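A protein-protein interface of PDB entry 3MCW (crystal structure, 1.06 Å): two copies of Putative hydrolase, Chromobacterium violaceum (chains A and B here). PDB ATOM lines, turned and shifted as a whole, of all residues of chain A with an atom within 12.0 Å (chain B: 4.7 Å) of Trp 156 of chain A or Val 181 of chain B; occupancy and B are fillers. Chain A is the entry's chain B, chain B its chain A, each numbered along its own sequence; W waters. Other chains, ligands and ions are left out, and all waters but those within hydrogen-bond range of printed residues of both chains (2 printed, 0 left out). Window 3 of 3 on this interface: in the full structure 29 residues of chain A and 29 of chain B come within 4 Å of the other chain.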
ATOM      1  N   ASP A 152      14.283  -3.152  29.281  1.00  0.00           N
ATOM      2  CA  ASP A 152      13.261  -2.591  28.398  1.00  0.00           C
ATOM      3  C   ASP A 152      13.462  -1.085  28.259  1.00  0.00           C
ATOM      4  O   ASP A 152      13.820  -0.405  29.217  1.00  0.00           O
ATOM      5  CB  ASP A 152      11.826  -2.797  28.938  1.00  0.00           C
ATOM      6  CG  ASP A 152      11.284  -4.209  28.832  1.00  0.00           C
ATOM      7  OD1 ASP A 152      12.075  -5.181  28.702  1.00  0.00           O
ATOM      8  OD2 ASP A 152      10.041  -4.308  28.948  1.00  0.00           O
ATOM      9  N   LYS A 153      13.172  -0.550  27.079  1.00  0.00           N
ATOM     10  CA  LYS A 153      13.345   0.877  26.822  1.00  0.00           C
ATOM     11  C   LYS A 153      12.361   1.325  25.765  1.00  0.00           C
ATOM     12  O   LYS A 153      12.168   0.632  24.757  1.00  0.00           O
ATOM     13  CB  LYS A 153      14.781   1.159  26.377  1.00  0.00           C
ATOM     14  CG  LYS A 153      15.115   2.650  26.311  1.00  0.00           C
ATOM     15  CD  LYS A 153      16.568   2.927  26.486  1.00  0.00           C
ATOM     16  CE  LYS A 153      16.867   4.391  26.335  1.00  0.00           C
ATOM     17  NZ  LYS A 153      16.578   5.247  27.481  1.00  0.00           N
ATOM     18  N   THR A 154      11.742   2.477  25.978  1.00  0.00           N
ATOM     19  CA  THR A 154      10.866   3.069  24.962  1.00  0.00           C
ATOM     20  C   THR A 154      11.705   3.763  23.901  1.00  0.00           C
ATOM     21  O   THR A 154      12.588   4.569  24.233  1.00  0.00           O
ATOM     22  CB  THR A 154       9.929   4.075  25.613  1.00  0.00           C
ATOM     23  OG1 THR A 154       9.249   3.450  26.713  1.00  0.00           O
ATOM     24  CG2 THR A 154       8.930   4.628  24.601  1.00  0.00           C
ATOM     25  N   ASP A 155      11.475   3.446  22.629  1.00  0.00           N
ATOM     26  CA  ASP A 155      12.223   4.090  21.571  1.00  0.00           C
ATOM     27  C   ASP A 155      11.678   5.511  21.342  1.00  0.00           C
ATOM     28  O   ASP A 155      10.713   5.951  21.950  1.00  0.00           O
ATOM     29  CB  ASP A 155      12.306   3.240  20.291  1.00  0.00           C
ATOM     30  CG  ASP A 155      11.015   3.211  19.440  1.00  0.00           C
ATOM     31  OD1 ASP A 155      10.122   4.022  19.667  1.00  0.00           O
ATOM     32  OD2 ASP A 155      11.015   2.375  18.510  1.00  0.00           O
ATOM     33  N   TRP A 156      12.312   6.267  20.450  1.00  0.00           N
ATOM     34  CA  TRP A 156      11.983   7.681  20.296  1.00  0.00           C
ATOM     35  C   TRP A 156      10.602   7.865  19.673  1.00  0.00           C
ATOM     36  O   TRP A 156      10.038   8.952  19.766  1.00  0.00           O
ATOM     37  CB  TRP A 156      13.046   8.375  19.430  1.00  0.00           C
ATOM     38  CG  TRP A 156      13.036   9.831  19.542  1.00  0.00           C
ATOM     39  CD1 TRP A 156      12.693  10.788  18.578  1.00  0.00           C
ATOM     40  CD2 TRP A 156      13.373  10.553  20.703  1.00  0.00           C
ATOM     41  NE1 TRP A 156      12.818  12.011  19.099  1.00  0.00           N
ATOM     42  CE2 TRP A 156      13.274  11.923  20.389  1.00  0.00           C
ATOM     43  CE3 TRP A 156      13.806  10.184  21.973  1.00  0.00           C
ATOM     44  CZ2 TRP A 156      13.481  12.920  21.342  1.00  0.00           C
ATOM     45  CZ3 TRP A 156      14.030  11.165  22.911  1.00  0.00           C
ATOM     46  CH2 TRP A 156      13.901  12.512  22.581  1.00  0.00           C
ATOM     47  N   HIS A 157      10.091   6.840  19.005  1.00  0.00           N
ATOM     48  CA  HIS A 157       8.745   6.890  18.402  1.00  0.00           C
ATOM     49  C   HIS A 157       7.654   6.433  19.380  1.00  0.00           C
ATOM     50  O   HIS A 157       6.480   6.363  19.020  1.00  0.00           O
ATOM     51  CB  HIS A 157       8.772   6.026  17.141  1.00  0.00           C
ATOM     52  CG  HIS A 157       7.554   6.142  16.284  1.00  0.00           C
ATOM     53  ND1 HIS A 157       6.773   5.060  15.947  1.00  0.00           N
ATOM     54  CD2 HIS A 157       6.984   7.215  15.696  1.00  0.00           C
ATOM     55  CE1 HIS A 157       5.781   5.460  15.170  1.00  0.00           C
ATOM     56  NE2 HIS A 157       5.883   6.767  15.005  1.00  0.00           N
ATOM     57  N   GLY A 158       8.031   6.096  20.604  1.00  0.00           N
ATOM     58  CA  GLY A 158       7.067   5.714  21.644  1.00  0.00           C
ATOM     59  C   GLY A 158       6.756   4.229  21.707  1.00  0.00           C
ATOM     60  O   GLY A 158       5.778   3.858  22.361  1.00  0.00           O
ATOM     61  N   ARG A 159       7.562   3.391  21.070  1.00  0.00           N
ATOM     62  CA  ARG A 159       7.367   1.946  21.127  1.00  0.00           C
ATOM     63  C   ARG A 159       8.191   1.330  22.233  1.00  0.00           C
ATOM     64  O   ARG A 159       9.377   1.541  22.292  1.00  0.00           O
ATOM     65  CB  ARG A 159       7.752   1.307  19.809  1.00  0.00           C
ATOM     66  CG  ARG A 159       7.486  -0.190  19.715  1.00  0.00           C
ATOM     67  N   ARG A 160       7.573   0.546  23.108  1.00  0.00           N
ATOM     68  CA  ARG A 160       8.344  -0.236  24.055  1.00  0.00           C
ATOM     69  C   ARG A 160       9.130  -1.310  23.332  1.00  0.00           C
ATOM     70  O   ARG A 160       8.557  -2.129  22.636  1.00  0.00           O
ATOM     71  CB  ARG A 160       7.458  -0.917  25.117  1.00  0.00           C
ATOM     72  CG  ARG A 160       8.306  -1.827  26.071  1.00  0.00           C
ATOM     73  CD  ARG A 160       7.584  -2.842  26.943  1.00  0.00           C
ATOM     74  NE  ARG A 160       6.848  -2.096  27.944  1.00  0.00           N
ATOM     75  CZ  ARG A 160       7.110  -1.937  29.278  1.00  0.00           C
ATOM     76  NH1 ARG A 160       8.082  -2.501  29.977  1.00  0.00           N
ATOM     77  NH2 ARG A 160       6.312  -1.140  29.959  1.00  0.00           N
ATOM     78  N   ARG A 161      10.442  -1.324  23.538  1.00  0.00           N
ATOM     79  CA  ARG A 161      11.296  -2.410  23.091  1.00  0.00           C
ATOM     80  C   ARG A 161      11.674  -3.231  24.308  1.00  0.00           C
ATOM     81  O   ARG A 161      12.067  -2.704  25.344  1.00  0.00           O
ATOM     82  CB  ARG A 161      12.551  -1.840  22.410  1.00  0.00           C
ATOM     83  CG  ARG A 161      12.259  -1.080  21.132  1.00  0.00           C
ATOM     84  CD  ARG A 161      11.663  -1.974  20.086  1.00  0.00           C
ATOM     85  NE  ARG A 161      11.635  -1.343  18.791  1.00  0.00           N
ATOM     86  CZ  ARG A 161      10.868  -1.733  17.802  1.00  0.00           C
ATOM     87  NH1 ARG A 161       9.993  -2.715  17.970  1.00  0.00           N
ATOM     88  NH2 ARG A 161      10.956  -1.097  16.644  1.00  0.00           N
ATOM     89  N   SER A 162      11.546  -4.551  24.202  1.00  0.00           N
ATOM     90  CA  SER A 162      11.950  -5.413  25.312  1.00  0.00           C
ATOM     91  C   SER A 162      13.456  -5.347  25.505  1.00  0.00           C
ATOM     92  O   SER A 162      14.203  -5.032  24.580  1.00  0.00           O
ATOM     93  CB  SER A 162      11.578  -6.858  25.014  1.00  0.00           C
ATOM     94  OG  SER A 162      12.393  -7.402  23.980  1.00  0.00           O
ATOM     95  N   GLU A 165      15.188  -7.099  22.760  1.00  0.00           N
ATOM     96  CA  GLU A 165      15.261  -6.283  21.536  1.00  0.00           C
ATOM     97  C   GLU A 165      16.344  -5.204  21.631  1.00  0.00           C
ATOM     98  O   GLU A 165      17.056  -4.962  20.652  1.00  0.00           O
ATOM     99  CB  GLU A 165      13.893  -5.661  21.234  1.00  0.00           C
ATOM    100  CG  GLU A 165      12.880  -6.697  20.762  1.00  0.00           C
ATOM    101  CD  GLU A 165      11.485  -6.180  20.601  1.00  0.00           C
ATOM    102  OE1 GLU A 165      10.980  -5.423  21.449  1.00  0.00           O
ATOM    103  OE2 GLU A 165      10.834  -6.612  19.618  1.00  0.00           O
ATOM    104  N   VAL A 166      16.410  -4.551  22.779  1.00  0.00           N
ATOM    105  CA  VAL A 166      17.410  -3.504  23.026  1.00  0.00           C
ATOM    106  C   VAL A 166      18.802  -4.121  22.910  1.00  0.00           C
ATOM    107  O   VAL A 166      19.707  -3.572  22.250  1.00  0.00           O
ATOM    108  CB  VAL A 166      17.190  -2.826  24.365  1.00  0.00           C
ATOM    109  CG1 VAL A 166      18.287  -1.847  24.676  1.00  0.00           C
ATOM    110  CG2 VAL A 166      15.839  -2.133  24.409  1.00  0.00           C
ATOM    111  N   MET A 169      19.649  -5.121  19.260  1.00  0.00           N
ATOM    112  CA  MET A 169      19.967  -3.987  18.381  1.00  0.00           C
ATOM    113  C   MET A 169      21.379  -3.456  18.712  1.00  0.00           C
ATOM    114  O   MET A 169      22.152  -3.160  17.801  1.00  0.00           O
ATOM    115  CB  MET A 169      18.847  -2.915  18.440  1.00  0.00           C
ATOM    116  CG  MET A 169      17.545  -3.362  17.735  1.00  0.00           C
ATOM    117  SD  MET A 169      16.039  -2.061  17.716  1.00  0.00           S
ATOM    118  CE  MET A 169      16.679  -1.097  16.240  1.00  0.00           C
ATOM    119  N   LEU B 143      21.496  17.140  19.245  1.00  0.00           N
ATOM    120  CA  LEU B 143      21.500  16.269  18.081  1.00  0.00           C
ATOM    121  C   LEU B 143      20.299  16.625  17.226  1.00  0.00           C
ATOM    122  O   LEU B 143      19.146  16.448  17.660  1.00  0.00           O
ATOM    123  CB  LEU B 143      21.456  14.804  18.532  1.00  0.00           C
ATOM    124  CG  LEU B 143      21.476  13.801  17.396  1.00  0.00           C
ATOM    125  CD1 LEU B 143      22.685  13.934  16.509  1.00  0.00           C
ATOM    126  CD2 LEU B 143      21.462  12.392  17.992  1.00  0.00           C
ATOM    127  N   GLU B 145      18.054  15.635  14.903  1.00  0.00           N
ATOM    128  CA  GLU B 145      17.768  14.281  14.441  1.00  0.00           C
ATOM    129  C   GLU B 145      17.182  14.217  13.027  1.00  0.00           C
ATOM    130  O   GLU B 145      17.343  13.246  12.325  1.00  0.00           O
ATOM    131  CB  GLU B 145      16.915  13.501  15.451  1.00  0.00           C
ATOM    132  CG  GLU B 145      15.525  14.022  15.625  1.00  0.00           C
ATOM    133  CD  GLU B 145      14.538  13.488  14.597  1.00  0.00           C
ATOM    134  OE1 GLU B 145      14.741  12.377  14.063  1.00  0.00           O
ATOM    135  OE2 GLU B 145      13.533  14.197  14.350  1.00  0.00           O
ATOM    136  N   ALA B 168      15.202   5.344  15.722  1.00  0.00           N
ATOM    137  CA  ALA B 168      14.434   5.589  16.939  1.00  0.00           C
ATOM    138  C   ALA B 168      15.102   4.973  18.181  1.00  0.00           C
ATOM    139  O   ALA B 168      15.021   5.544  19.274  1.00  0.00           O
ATOM    140  CB  ALA B 168      13.033   5.046  16.774  1.00  0.00           C
ATOM    141  N   LEU B 171      18.263   7.173  18.970  1.00  0.00           N
ATOM    142  CA  LEU B 171      17.866   8.427  19.602  1.00  0.00           C
ATOM    143  C   LEU B 171      17.475   8.225  21.072  1.00  0.00           C
ATOM    144  O   LEU B 171      17.786   9.042  21.919  1.00  0.00           O
ATOM    145  CB  LEU B 171      16.722   9.110  18.854  1.00  0.00           C
ATOM    146  CG  LEU B 171      17.010   9.645  17.455  1.00  0.00           C
ATOM    147  CD1 LEU B 171      15.753  10.339  16.944  1.00  0.00           C
ATOM    148  CD2 LEU B 171      18.281  10.492  17.380  1.00  0.00           C
ATOM    149  N   ALA B 172      16.738   7.160  21.359  1.00  0.00           N
ATOM    150  CA  ALA B 172      16.339   6.890  22.732  1.00  0.00           C
ATOM    151  C   ALA B 172      17.548   6.624  23.630  1.00  0.00           C
ATOM    152  O   ALA B 172      17.557   7.047  24.784  1.00  0.00           O
ATOM    153  CB  ALA B 172      15.364   5.734  22.783  1.00  0.00           C
ATOM    154  N   ASP B 175      19.387  10.298  23.958  1.00  0.00           N
ATOM    155  CA  ASP B 175      18.723  11.414  24.597  1.00  0.00           C
ATOM    156  C   ASP B 175      18.850  11.322  26.103  1.00  0.00           C
ATOM    157  O   ASP B 175      18.683  10.255  26.701  1.00  0.00           O
ATOM    158  CB  ASP B 175      17.235  11.487  24.218  1.00  0.00           C
ATOM    159  CG  ASP B 175      16.615  12.753  24.711  1.00  0.00           C
ATOM    160  OD1 ASP B 175      17.095  13.855  24.343  1.00  0.00           O
ATOM    161  OD2 ASP B 175      15.686  12.700  25.579  1.00  0.00           O
ATOM    162  N   CYS B 179      23.053  13.542  25.166  1.00  0.00           N
ATOM    163  CA  CYS B 179      22.737  14.752  24.391  1.00  0.00           C
ATOM    164  C   CYS B 179      21.280  15.103  24.568  1.00  0.00           C
ATOM    165  O   CYS B 179      20.529  14.388  25.246  1.00  0.00           O
ATOM    166  CB  CYS B 179      23.027  14.531  22.909  1.00  0.00           C
ATOM    167  SG  CYS B 179      21.870  13.392  22.108  1.00  0.00           S
ATOM    168  N   ARG B 180      20.887  16.250  24.016  1.00  0.00           N
ATOM    169  CA  ARG B 180      19.485  16.601  23.849  1.00  0.00           C
ATOM    170  C   ARG B 180      19.124  16.379  22.391  1.00  0.00           C
ATOM    171  O   ARG B 180      19.672  17.038  21.496  1.00  0.00           O
ATOM    172  CB  ARG B 180      19.268  18.059  24.230  1.00  0.00           C
ATOM    173  CG  ARG B 180      17.815  18.466  24.136  1.00  0.00           C
ATOM    174  CD  ARG B 180      17.586  19.860  24.643  1.00  0.00           C
ATOM    175  NE  ARG B 180      16.209  20.250  24.456  1.00  0.00           N
ATOM    176  CZ  ARG B 180      15.650  21.280  25.055  1.00  0.00           C
ATOM    177  NH1 ARG B 180      16.375  22.044  25.851  1.00  0.00           N
ATOM    178  NH2 ARG B 180      14.386  21.553  24.814  1.00  0.00           N
ATOM    179  N   VAL B 181      18.178  15.482  22.131  1.00  0.00           N
ATOM    180  CA  VAL B 181      17.680  15.248  20.774  1.00  0.00           C
ATOM    181  C   VAL B 181      16.643  16.334  20.459  1.00  0.00           C
ATOM    182  O   VAL B 181      15.724  16.555  21.215  1.00  0.00           O
ATOM    183  CB  VAL B 181      17.070  13.852  20.676  1.00  0.00           C
ATOM    184  CG1 VAL B 181      16.385  13.675  19.301  1.00  0.00           C
ATOM    185  CG2 VAL B 181      18.150  12.795  20.904  1.00  0.00           C
ATOM    186  N   CYS B 182      16.812  17.000  19.311  1.00  0.00           N
ATOM    187  CA  CYS B 182      15.846  17.993  18.918  1.00  0.00           C
ATOM    188  C   CYS B 182      15.786  18.114  17.411  1.00  0.00           C
ATOM    189  O   CYS B 182      16.380  17.300  16.690  1.00  0.00           O
ATOM    190  CB  CYS B 182      16.235  19.299  19.556  1.00  0.00           C
ATOM    191  SG  CYS B 182      17.882  19.777  19.035  1.00  0.00           S
HETATM  192  O   HOH W   1      18.319   7.479  27.648  1.00  0.00           O
HETATM  193  O   HOH W   2      12.215  14.220  17.267  1.00  0.00           O
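The backbone carbonyl oxygen (O) of Ala 172 of chain B sits close to the side-chain amino group (NZ) of Lys 153 of chain A, 3.4 Å away. The backbone NH of Trp 156 of chain A is in hydrogen-bond range of the backbone carbonyl oxygen of Ala 168 of chain B (3.0 Å).
O of Lys 153 of chain A is in hydrogen-bond range of N of Arg 161 of chain A (2.9 Å). N of Gly 158 of chain A lies within hydrogen-bond range of OD1 of Asp 155 of chain A (3.1 Å). The side-chain carboxylate (OD1) of Asp 155 of chain A lies within hydrogen-bond range of the backbone NH (N) of His 157 of chain A, 2.9 Å away. N of Arg 159 of chain A lies within hydrogen-bond range of OD1 of Asp 155 of chain A, 3.0 Å away. The guanidinium group of Arg 161 of chain A is in salt-bridge range of the side-chain carboxylate of Asp 155 of chain A, at 3.8 Å. The backbone NH (N) of Val 181 of chain B sits at hydrogen-bond distance from the side-chain carboxylate (OD1) of Asp 175 of chain B, at 3.0 Å.
Ala 172 of chain B touches Thr 154 of chain A (CB to O, 3.3 Å). O of Ala 168 of chain B touches CB of Asp 155 of chain A (3.7 Å). CA of Asp 155 of chain A touches CB of Ala 172 of chain B, 3.7 Å away. Trp 156 of chain A touches Leu 171 of chain B. Trp 156 of chain A touches Ala 172 of chain B. Trp 156 of chain A touches Asp 175 of chain B (CH2 to CG, 3.5 Å). CG1 of Val 181 of chain B touches CZ2 of Trp 156 of chain A, 3.6 Å away.
Printed residues of chain B within 4 Å of Thr 154 of chain A: Ala 172. Of the printed residues of chain B, Asp 155 of chain A touches Ala 168 and Ala 172. Trp 156 of chain A touches five residues of chain B. No residue of chain A comes within 4 Å of Glu 145 of chain B. Of chain A, only Asp 155 (3.7 Å) and Trp 156 (3.0 Å) come within 4 Å of Ala 168 of chain B. Of the printed residues of chain A, Asp 175 of chain B touches Trp 156 (3.5 Å). No residue of chain A comes within 4 Å of Cys 179 of chain B. Of the printed residues of chain A, Val 181 of chain B touches Trp 156 (3.6 Å). The nearest printed residue of chain B that does not touch Trp 156 of chain A is Glu 145 of chain B (4.8 Å). The nearest residue of chain A that does not touch Val 181 of chain B is His 157 of chain A (9.3 Å).
Hydrophobic or aromatic side chains of chain B that line the printed part of chain A: Ala 168, Leu 171, Ala 172 and Val 181. Printed residues of chain A that touch a printed residue of chain B: Lys 153, Thr 154, Asp 155 and Trp 156. Hydrophobic or aromatic side chains of chain A within 4 Å of the printed part of chain B: Trp 156. Among the printed residues, 9 pairs touch across the chains. Among the printed residues, no Asp or Glu carboxylate lies within 4 Å of a Lys or Arg side-chain nitrogen of the other chain.
No position is printed for both chains.
Water W1 lies within hydrogen-bond range of the side-chain amino group (NZ) of Lys 153 of chain A (2.8 Å), the backbone carbonyl oxygen (O) of Asp 175 of chain B (3.0 Å) and the backbone carbonyl oxygen (O) of Ala 172 of chain B (3.0 Å). Water W2 lies within hydrogen-bond range of NE1 of Trp 156 of chain A (2.9 Å) and OE2 of Glu 145 of chain B (3.2 Å).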
